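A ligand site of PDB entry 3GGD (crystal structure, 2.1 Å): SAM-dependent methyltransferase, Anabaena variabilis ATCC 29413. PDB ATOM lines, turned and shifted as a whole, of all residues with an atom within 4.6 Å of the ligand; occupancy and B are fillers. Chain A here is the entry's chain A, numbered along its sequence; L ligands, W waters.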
ATOM      1  N   VAL A  15      -4.789 -15.022 -16.183  1.00  0.00           N
ATOM      2  CA  VAL A  15      -5.779 -15.266 -15.169  1.00  0.00           C
ATOM      3  C   VAL A  15      -5.819 -16.747 -14.722  1.00  0.00           C
ATOM      4  O   VAL A  15      -5.837 -17.026 -13.506  1.00  0.00           O
ATOM      5  CB  VAL A  15      -7.180 -14.768 -15.650  1.00  0.00           C
ATOM      6  CG1 VAL A  15      -8.331 -15.255 -14.696  1.00  0.00           C
ATOM      7  CG2 VAL A  15      -7.177 -13.228 -15.830  1.00  0.00           C
ATOM      8  N   TRP A  19      -4.658 -17.949 -10.779  1.00  0.00           N
ATOM      9  CA  TRP A  19      -5.608 -18.626  -9.909  1.00  0.00           C
ATOM     10  C   TRP A  19      -5.202 -20.045  -9.542  1.00  0.00           C
ATOM     11  O   TRP A  19      -5.393 -20.476  -8.399  1.00  0.00           O
ATOM     12  CB  TRP A  19      -7.025 -18.596 -10.490  1.00  0.00           C
ATOM     13  CG  TRP A  19      -7.710 -17.288 -10.222  1.00  0.00           C
ATOM     14  CD1 TRP A  19      -7.828 -16.230 -11.094  1.00  0.00           C
ATOM     15  CD2 TRP A  19      -8.274 -16.869  -8.980  1.00  0.00           C
ATOM     16  NE1 TRP A  19      -8.464 -15.184 -10.453  1.00  0.00           N
ATOM     17  CE2 TRP A  19      -8.765 -15.560  -9.176  1.00  0.00           C
ATOM     18  CE3 TRP A  19      -8.421 -17.482  -7.737  1.00  0.00           C
ATOM     19  CZ2 TRP A  19      -9.419 -14.850  -8.170  1.00  0.00           C
ATOM     20  CZ3 TRP A  19      -9.067 -16.776  -6.734  1.00  0.00           C
ATOM     21  CH2 TRP A  19      -9.545 -15.478  -6.948  1.00  0.00           C
ATOM     22  N   TRP A  23      -4.530 -21.391  -5.773  1.00  0.00           N
ATOM     23  CA  TRP A  23      -5.227 -22.567  -5.250  1.00  0.00           C
ATOM     24  C   TRP A  23      -4.269 -23.675  -4.952  1.00  0.00           C
ATOM     25  O   TRP A  23      -4.419 -24.369  -3.947  1.00  0.00           O
ATOM     26  CB  TRP A  23      -6.324 -23.021  -6.185  1.00  0.00           C
ATOM     27  CG  TRP A  23      -7.605 -22.261  -6.050  1.00  0.00           C
ATOM     28  CD1 TRP A  23      -8.223 -21.509  -7.026  1.00  0.00           C
ATOM     29  CD2 TRP A  23      -8.463 -22.187  -4.891  1.00  0.00           C
ATOM     30  NE1 TRP A  23      -9.399 -20.998  -6.551  1.00  0.00           N
ATOM     31  CE2 TRP A  23      -9.558 -21.388  -5.243  1.00  0.00           C
ATOM     32  CE3 TRP A  23      -8.396 -22.731  -3.604  1.00  0.00           C
ATOM     33  CZ2 TRP A  23     -10.609 -21.144  -4.366  1.00  0.00           C
ATOM     34  CZ3 TRP A  23      -9.427 -22.461  -2.706  1.00  0.00           C
ATOM     35  CH2 TRP A  23     -10.528 -21.681  -3.084  1.00  0.00           C
ATOM     36  N   TRP A  35     -12.600 -15.287   1.041  1.00  0.00           N
ATOM     37  CA  TRP A  35     -14.052 -15.254   0.761  1.00  0.00           C
ATOM     38  C   TRP A  35     -14.822 -16.488   1.261  1.00  0.00           C
ATOM     39  O   TRP A  35     -16.046 -16.551   1.111  1.00  0.00           O
ATOM     40  CB  TRP A  35     -14.284 -15.141  -0.739  1.00  0.00           C
ATOM     41  CG  TRP A  35     -13.525 -16.197  -1.471  1.00  0.00           C
ATOM     42  CD1 TRP A  35     -13.898 -17.489  -1.695  1.00  0.00           C
ATOM     43  CD2 TRP A  35     -12.225 -16.039  -2.024  1.00  0.00           C
ATOM     44  NE1 TRP A  35     -12.889 -18.161  -2.370  1.00  0.00           N
ATOM     45  CE2 TRP A  35     -11.853 -17.284  -2.586  1.00  0.00           C
ATOM     46  CE3 TRP A  35     -11.333 -14.973  -2.115  1.00  0.00           C
ATOM     47  CZ2 TRP A  35     -10.627 -17.473  -3.225  1.00  0.00           C
ATOM     48  CZ3 TRP A  35     -10.117 -15.163  -2.744  1.00  0.00           C
ATOM     49  CH2 TRP A  35      -9.777 -16.412  -3.288  1.00  0.00           C
ATOM     50  N   ASP A  62     -22.662 -23.942 -10.554  1.00  0.00           N
ATOM     51  CA  ASP A  62     -21.911 -23.053  -9.616  1.00  0.00           C
ATOM     52  C   ASP A  62     -20.693 -22.649 -10.412  1.00  0.00           C
ATOM     53  O   ASP A  62     -19.748 -23.435 -10.565  1.00  0.00           O
ATOM     54  CB  ASP A  62     -21.503 -23.751  -8.311  1.00  0.00           C
ATOM     55  CG  ASP A  62     -20.887 -22.808  -7.290  1.00  0.00           C
ATOM     56  OD1 ASP A  62     -20.554 -21.654  -7.636  1.00  0.00           O
ATOM     57  OD2 ASP A  62     -20.727 -23.233  -6.118  1.00  0.00           O
ATOM     58  N   PHE A  63     -20.764 -21.466 -11.013  1.00  0.00           N
ATOM     59  CA  PHE A  63     -19.729 -21.001 -11.920  1.00  0.00           C
ATOM     60  C   PHE A  63     -18.590 -20.342 -11.121  1.00  0.00           C
ATOM     61  O   PHE A  63     -18.846 -19.410 -10.359  1.00  0.00           O
ATOM     62  CB  PHE A  63     -20.276 -19.946 -12.902  1.00  0.00           C
ATOM     63  CG  PHE A  63     -19.331 -19.683 -13.992  1.00  0.00           C
ATOM     64  CD1 PHE A  63     -18.249 -18.838 -13.788  1.00  0.00           C
ATOM     65  CD2 PHE A  63     -19.422 -20.405 -15.171  1.00  0.00           C
ATOM     66  CE1 PHE A  63     -17.299 -18.663 -14.769  1.00  0.00           C
ATOM     67  CE2 PHE A  63     -18.466 -20.225 -16.183  1.00  0.00           C
ATOM     68  CZ  PHE A  63     -17.382 -19.367 -15.958  1.00  0.00           C
ATOM     69  N   ALA A  64     -17.358 -20.831 -11.295  1.00  0.00           N
ATOM     70  CA  ALA A  64     -16.182 -20.359 -10.498  1.00  0.00           C
ATOM     71  C   ALA A  64     -16.409 -20.780  -9.024  1.00  0.00           C
ATOM     72  O   ALA A  64     -16.370 -19.977  -8.076  1.00  0.00           O
ATOM     73  CB  ALA A  64     -15.930 -18.805 -10.654  1.00  0.00           C
ATOM     74  N   CYS A  65     -16.692 -22.058  -8.854  1.00  0.00           N
ATOM     75  CA  CYS A  65     -17.075 -22.627  -7.570  1.00  0.00           C
ATOM     76  C   CYS A  65     -15.972 -22.715  -6.505  1.00  0.00           C
ATOM     77  O   CYS A  65     -16.248 -23.057  -5.335  1.00  0.00           O
ATOM     78  CB  CYS A  65     -17.671 -24.021  -7.804  1.00  0.00           C
ATOM     79  SG  CYS A  65     -16.444 -25.222  -8.462  1.00  0.00           S
ATOM     80  N   GLY A  66     -14.717 -22.480  -6.902  1.00  0.00           N
ATOM     81  CA  GLY A  66     -13.615 -22.525  -5.929  1.00  0.00           C
ATOM     82  C   GLY A  66     -13.541 -23.898  -5.275  1.00  0.00           C
ATOM     83  O   GLY A  66     -13.637 -24.936  -5.953  1.00  0.00           O
ATOM     84  N   ASN A  67     -13.405 -23.910  -3.946  1.00  0.00           N
ATOM     85  CA  ASN A  67     -13.287 -25.149  -3.184  1.00  0.00           C
ATOM     86  C   ASN A  67     -14.599 -25.808  -2.827  1.00  0.00           C
ATOM     87  O   ASN A  67     -14.633 -26.764  -2.035  1.00  0.00           O
ATOM     88  CB  ASN A  67     -12.458 -24.945  -1.902  1.00  0.00           C
ATOM     89  CG  ASN A  67     -13.079 -23.930  -0.965  1.00  0.00           C
ATOM     90  OD1 ASN A  67     -14.119 -23.377  -1.260  1.00  0.00           O
ATOM     91  ND2 ASN A  67     -12.420 -23.677   0.150  1.00  0.00           N
ATOM     92  N   GLN A  70     -19.878 -23.529  -1.169  1.00  0.00           N
ATOM     93  CA  GLN A  70     -21.276 -23.150  -1.438  1.00  0.00           C
ATOM     94  C   GLN A  70     -21.996 -24.204  -2.267  1.00  0.00           C
ATOM     95  O   GLN A  70     -23.233 -24.397  -2.155  1.00  0.00           O
ATOM     96  CB  GLN A  70     -21.345 -21.778  -2.117  1.00  0.00           C
ATOM     97  CG  GLN A  70     -20.490 -20.640  -1.435  1.00  0.00           C
ATOM     98  CD  GLN A  70     -20.714 -20.481   0.080  1.00  0.00           C
ATOM     99  OE1 GLN A  70     -21.854 -20.526   0.558  1.00  0.00           O
ATOM    100  NE2 GLN A  70     -19.623 -20.246   0.830  1.00  0.00           N
ATOM    101  N   ASP A  85     -14.699 -24.567 -12.464  1.00  0.00           N
ATOM    102  CA  ASP A  85     -13.649 -23.655 -12.084  1.00  0.00           C
ATOM    103  C   ASP A  85     -12.476 -23.831 -13.036  1.00  0.00           C
ATOM    104  O   ASP A  85     -12.247 -24.944 -13.572  1.00  0.00           O
ATOM    105  CB  ASP A  85     -13.217 -23.875 -10.622  1.00  0.00           C
ATOM    106  CG  ASP A  85     -12.568 -22.631 -10.012  1.00  0.00           C
ATOM    107  OD1 ASP A  85     -11.350 -22.401 -10.271  1.00  0.00           O
ATOM    108  OD2 ASP A  85     -13.285 -21.873  -9.296  1.00  0.00           O
ATOM    109  N   VAL A  86     -11.725 -22.761 -13.224  1.00  0.00           N
ATOM    110  CA  VAL A  86     -10.502 -22.789 -14.034  1.00  0.00           C
ATOM    111  C   VAL A  86      -9.357 -23.556 -13.388  1.00  0.00           C
ATOM    112  O   VAL A  86      -8.474 -24.038 -14.092  1.00  0.00           O
ATOM    113  CB  VAL A  86     -10.000 -21.335 -14.365  1.00  0.00           C
ATOM    114  CG1 VAL A  86      -9.339 -20.657 -13.155  1.00  0.00           C
ATOM    115  CG2 VAL A  86      -9.075 -21.321 -15.590  1.00  0.00           C
ATOM    116  N   SER A  87      -9.386 -23.703 -12.047  1.00  0.00           N
ATOM    117  CA  SER A  87      -8.273 -24.248 -11.315  1.00  0.00           C
ATOM    118  C   SER A  87      -8.448 -25.705 -10.938  1.00  0.00           C
ATOM    119  O   SER A  87      -9.387 -26.047 -10.192  1.00  0.00           O
ATOM    120  CB  SER A  87      -8.047 -23.454 -10.000  1.00  0.00           C
ATOM    121  OG  SER A  87      -7.098 -24.105  -9.138  1.00  0.00           O
ATOM    122  N   LEU A 108     -13.210 -25.688 -16.266  1.00  0.00           N
ATOM    123  CA  LEU A 108     -13.653 -24.803 -17.339  1.00  0.00           C
ATOM    124  C   LEU A 108     -13.053 -23.427 -17.142  1.00  0.00           C
ATOM    125  O   LEU A 108     -13.024 -22.893 -16.024  1.00  0.00           O
ATOM    126  CB  LEU A 108     -15.195 -24.695 -17.455  1.00  0.00           C
ATOM    127  CG  LEU A 108     -15.771 -23.712 -18.525  1.00  0.00           C
ATOM    128  CD1 LEU A 108     -17.015 -24.296 -19.261  1.00  0.00           C
ATOM    129  CD2 LEU A 108     -16.100 -22.395 -17.910  1.00  0.00           C
ATOM    130  N   ASP A 109     -12.608 -22.852 -18.245  1.00  0.00           N
ATOM    131  CA  ASP A 109     -12.078 -21.515 -18.276  1.00  0.00           C
ATOM    132  C   ASP A 109     -13.069 -20.586 -18.941  1.00  0.00           C
ATOM    133  O   ASP A 109     -13.261 -20.647 -20.156  1.00  0.00           O
ATOM    134  CB  ASP A 109     -10.718 -21.509 -19.036  1.00  0.00           C
ATOM    135  CG  ASP A 109      -9.979 -20.158 -18.926  1.00  0.00           C
ATOM    136  OD1 ASP A 109     -10.642 -19.127 -18.662  1.00  0.00           O
ATOM    137  OD2 ASP A 109      -8.740 -20.154 -19.081  1.00  0.00           O
ATOM    138  N   GLY A 110     -13.658 -19.683 -18.138  1.00  0.00           N
ATOM    139  CA  GLY A 110     -14.631 -18.714 -18.604  1.00  0.00           C
ATOM    140  C   GLY A 110     -14.136 -17.739 -19.685  1.00  0.00           C
ATOM    141  O   GLY A 110     -14.944 -17.106 -20.373  1.00  0.00           O
ATOM    142  N   LEU A 111     -12.805 -17.639 -19.826  1.00  0.00           N
ATOM    143  CA  LEU A 111     -12.207 -16.762 -20.804  1.00  0.00           C
ATOM    144  C   LEU A 111     -11.981 -17.507 -22.110  1.00  0.00           C
ATOM    145  O   LEU A 111     -11.466 -16.914 -23.036  1.00  0.00           O
ATOM    146  CB  LEU A 111     -10.897 -16.131 -20.272  1.00  0.00           C
ATOM    147  CG  LEU A 111     -11.089 -15.322 -18.968  1.00  0.00           C
ATOM    148  CD1 LEU A 111      -9.729 -14.644 -18.568  1.00  0.00           C
ATOM    149  CD2 LEU A 111     -12.192 -14.270 -19.125  1.00  0.00           C
ATOM    150  N   ARG A 131     -20.718 -16.604  -7.299  1.00  0.00           N
ATOM    151  CA  ARG A 131     -20.338 -15.794  -6.139  1.00  0.00           C
ATOM    152  C   ARG A 131     -18.897 -15.301  -6.329  1.00  0.00           C
ATOM    153  O   ARG A 131     -17.907 -16.063  -6.230  1.00  0.00           O
ATOM    154  CB  ARG A 131     -20.485 -16.634  -4.868  1.00  0.00           C
ATOM    155  CG  ARG A 131     -20.186 -15.831  -3.600  1.00  0.00           C
ATOM    156  CD  ARG A 131     -20.464 -16.671  -2.332  1.00  0.00           C
ATOM    157  NE  ARG A 131     -20.269 -15.886  -1.111  1.00  0.00           N
ATOM    158  CZ  ARG A 131     -19.139 -15.876  -0.412  1.00  0.00           C
ATOM    159  NH1 ARG A 131     -18.108 -16.602  -0.806  1.00  0.00           N
ATOM    160  NH2 ARG A 131     -19.051 -15.146   0.698  1.00  0.00           N
ATOM    161  N   THR A 132     -18.794 -14.007  -6.593  1.00  0.00           N
ATOM    162  CA  THR A 132     -17.553 -13.312  -6.849  1.00  0.00           C
ATOM    163  C   THR A 132     -16.734 -13.951  -7.958  1.00  0.00           C
ATOM    164  O   THR A 132     -15.576 -14.288  -7.796  1.00  0.00           O
ATOM    165  CB  THR A 132     -16.748 -13.043  -5.573  1.00  0.00           C
ATOM    166  OG1 THR A 132     -16.622 -14.243  -4.772  1.00  0.00           O
ATOM    167  CG2 THR A 132     -17.459 -11.900  -4.753  1.00  0.00           C
ATOM    168  N   HIS A 136     -12.971  -9.549 -10.028  1.00  0.00           N
ATOM    169  CA  HIS A 136     -11.510  -9.632 -10.134  1.00  0.00           C
ATOM    170  C   HIS A 136     -10.999  -9.823 -11.566  1.00  0.00           C
ATOM    171  O   HIS A 136      -9.780  -9.772 -11.801  1.00  0.00           O
ATOM    172  CB  HIS A 136     -10.994 -10.796  -9.266  1.00  0.00           C
ATOM    173  CG  HIS A 136     -11.665 -12.077  -9.576  1.00  0.00           C
ATOM    174  ND1 HIS A 136     -11.325 -12.843 -10.677  1.00  0.00           N
ATOM    175  CD2 HIS A 136     -12.677 -12.727  -8.949  1.00  0.00           C
ATOM    176  CE1 HIS A 136     -12.110 -13.911 -10.710  1.00  0.00           C
ATOM    177  NE2 HIS A 136     -12.939 -13.850  -9.678  1.00  0.00           N
ATOM    178  N   ILE A 137     -11.906 -10.074 -12.514  1.00  0.00           N
ATOM    179  CA  ILE A 137     -11.487 -10.258 -13.903  1.00  0.00           C
ATOM    180  C   ILE A 137     -11.005  -8.930 -14.491  1.00  0.00           C
ATOM    181  O   ILE A 137     -11.695  -7.905 -14.404  1.00  0.00           O
ATOM    182  CB  ILE A 137     -12.622 -10.873 -14.782  1.00  0.00           C
ATOM    183  CG1 ILE A 137     -13.067 -12.245 -14.231  1.00  0.00           C
ATOM    184  CG2 ILE A 137     -12.200 -10.980 -16.276  1.00  0.00           C
ATOM    185  CD1 ILE A 137     -12.107 -13.424 -14.479  1.00  0.00           C
HETATM  186  N1  LIG L   1     -17.510 -18.817  -5.907  1.00  0.00           N
HETATM  187  C1  LIG L   1     -16.473 -19.306  -4.963  1.00  0.00           C
HETATM  188  C2  LIG L   1     -15.061 -18.781  -5.280  1.00  0.00           C
HETATM  189  C3  LIG L   1     -14.815 -17.267  -5.379  1.00  0.00           C
HETATM  190  S1  LIG L   1     -13.087 -16.846  -5.660  1.00  0.00           S
HETATM  191  C4  LIG L   1     -16.821 -18.957  -3.514  1.00  0.00           C
HETATM  192  O1  LIG L   1     -16.306 -19.604  -2.575  1.00  0.00           O
HETATM  193  O2  LIG L   1     -17.595 -18.031  -3.273  1.00  0.00           O
HETATM  194  C5  LIG L   1     -13.072 -16.651  -7.418  1.00  0.00           C
HETATM  195  C6  LIG L   1     -13.020 -18.021  -8.172  1.00  0.00           C
HETATM  196  O3  LIG L   1     -13.046 -17.787  -9.593  1.00  0.00           O
HETATM  197  C7  LIG L   1     -11.772 -18.891  -7.937  1.00  0.00           C
HETATM  198  O4  LIG L   1     -12.098 -20.211  -7.532  1.00  0.00           O
HETATM  199  C8  LIG L   1     -11.080 -18.935  -9.299  1.00  0.00           C
HETATM  200  O5  LIG L   1     -10.242 -20.085  -9.540  1.00  0.00           O
HETATM  201  C9  LIG L   1     -12.249 -18.769 -10.247  1.00  0.00           C
HETATM  202  N2  LIG L   1     -11.862 -18.331 -11.594  1.00  0.00           N
HETATM  203  C10 LIG L   1     -10.958 -17.352 -11.852  1.00  0.00           C
HETATM  204  N3  LIG L   1     -10.849 -17.170 -13.184  1.00  0.00           N
HETATM  205  C11 LIG L   1     -11.705 -18.058 -13.769  1.00  0.00           C
HETATM  206  C12 LIG L   1     -12.021 -18.413 -15.148  1.00  0.00           C
HETATM  207  N4  LIG L   1     -11.360 -17.724 -16.114  1.00  0.00           N
HETATM  208  N5  LIG L   1     -12.911 -19.390 -15.408  1.00  0.00           N
HETATM  209  C13 LIG L   1     -13.514 -20.067 -14.380  1.00  0.00           C
HETATM  210  N6  LIG L   1     -13.230 -19.786 -13.103  1.00  0.00           N
HETATM  211  C14 LIG L   1     -12.343 -18.840 -12.742  1.00  0.00           C
HETATM  212  O   HOH W   1     -19.644 -19.198  -7.802  1.00  0.00           O
HETATM  213  O   HOH W   2     -16.952 -20.189  -0.179  1.00  0.00           O
HETATM  214  O   HOH W   3     -18.023 -22.309  -3.248  1.00  0.00           O
HETATM  215  O   HOH W   4     -13.905 -20.972  -2.615  1.00  0.00           O
HETATM  216  O   HOH W   5     -19.535 -20.754  -5.012  1.00  0.00           O
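The side-chain carboxylate of Asp 85 lies within hydrogen-bond range of the backbone NH of Ser 87 (3.0 Å).
O of Thr 132 is in hydrogen-bond range of NE2 of His 136 (3.3 Å).
The backbone NH of Cys 65 is in hydrogen-bond range of the side-chain carboxylate of Asp 85 (3.4 Å).
The side-chain carboxylate (OD2) of Asp 85 sits at hydrogen-bond distance from the backbone NH (N) of Gly 66 (2.9 Å).
O of Trp 35 is in hydrogen-bond range of NH1 of Arg 131, at 2.8 Å.
O of Leu 108 is in hydrogen-bond range of N of Val 86, at 3.1 Å.
The backbone carbonyl oxygen of Asp 85 sits at hydrogen-bond distance from the backbone NH of Leu 108 (3.0 Å).
The side-chain carboxylate of Asp 109 sits at hydrogen-bond distance from the backbone NH of Leu 111 (2.9 Å).
Water W2 bridges O1 of the ligand and NE2 of Gln 70.
Water W4 lies within hydrogen-bond range of O1 of the ligand (2.8 Å), OD1 of Asn 67 (2.8 Å) and NE1 of Trp 35 (3.0 Å).
Water W5 lies within hydrogen-bond range of N1 of the ligand and OD1 of Asp 62.
Water W3 lies within hydrogen-bond range of the backbone carbonyl oxygen (O) of Cys 65, the backbone NH (N) of Gln 70 and an oxygen (O1) of the ligand.
An oxygen (O2) of the ligand lies within salt-bridge range of the guanidinium group (NH1) of Arg 131, 2.9 Å away.
N4 of the ligand is in hydrogen-bond range of OD1 of Asp 109.
A nitrogen (N1) of the ligand is in hydrogen-bond range of the backbone carbonyl oxygen (O) of Arg 131 (2.8 Å).
OD1 of Asp 85 lies within hydrogen-bond range of O5 of the ligand.
N6 of the ligand lies within hydrogen-bond range of N of Val 86.
The indole nitrogen of Trp 35 lies close to a sulfur (S1) of the ligand, 3.5 Å away.
The indole nitrogen (NE1) of Trp 23 sits at hydrogen-bond distance from an oxygen (O4) of the ligand (3.0 Å).
The backbone carbonyl oxygen (O) of Ala 64 sits at hydrogen-bond distance from a nitrogen (N1) of the ligand (2.7 Å).
The backbone NH of Gly 110 sits at hydrogen-bond distance from a nitrogen (N5) of the ligand (2.8 Å).
Val 15 touches the ligand.
Trp 19 touches the ligand (CE3 to C8, 3.4 Å).
C of Cys 65 touches C1 of the ligand, 3.8 Å away.
Gly 66 touches the ligand (CA to O4, 3.2 Å).
Leu 108 touches the ligand (O to C13, 3.3 Å).
CG of Leu 111 touches N4 of the ligand, at 3.7 Å.
O of Thr 132 touches C5 of the ligand (3.5 Å).
NE2 of His 136 touches C5 of the ligand, 3.6 Å away.
Hydrophobic or aromatic side chains within 4 Å of the ligand: Val 15, Trp 19, Trp 23, Trp 35, Ala 64, Val 86, Leu 111 and His 136.
16 residues have an atom within 4 Å of the ligand: Val 15, Trp 19, Trp 23, Trp 35, Ala 64, Cys 65, Gly 66, Asp 85, Val 86, Leu 108, Asp 109, Gly 110, Leu 111, Arg 131, Thr 132 and His 136.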
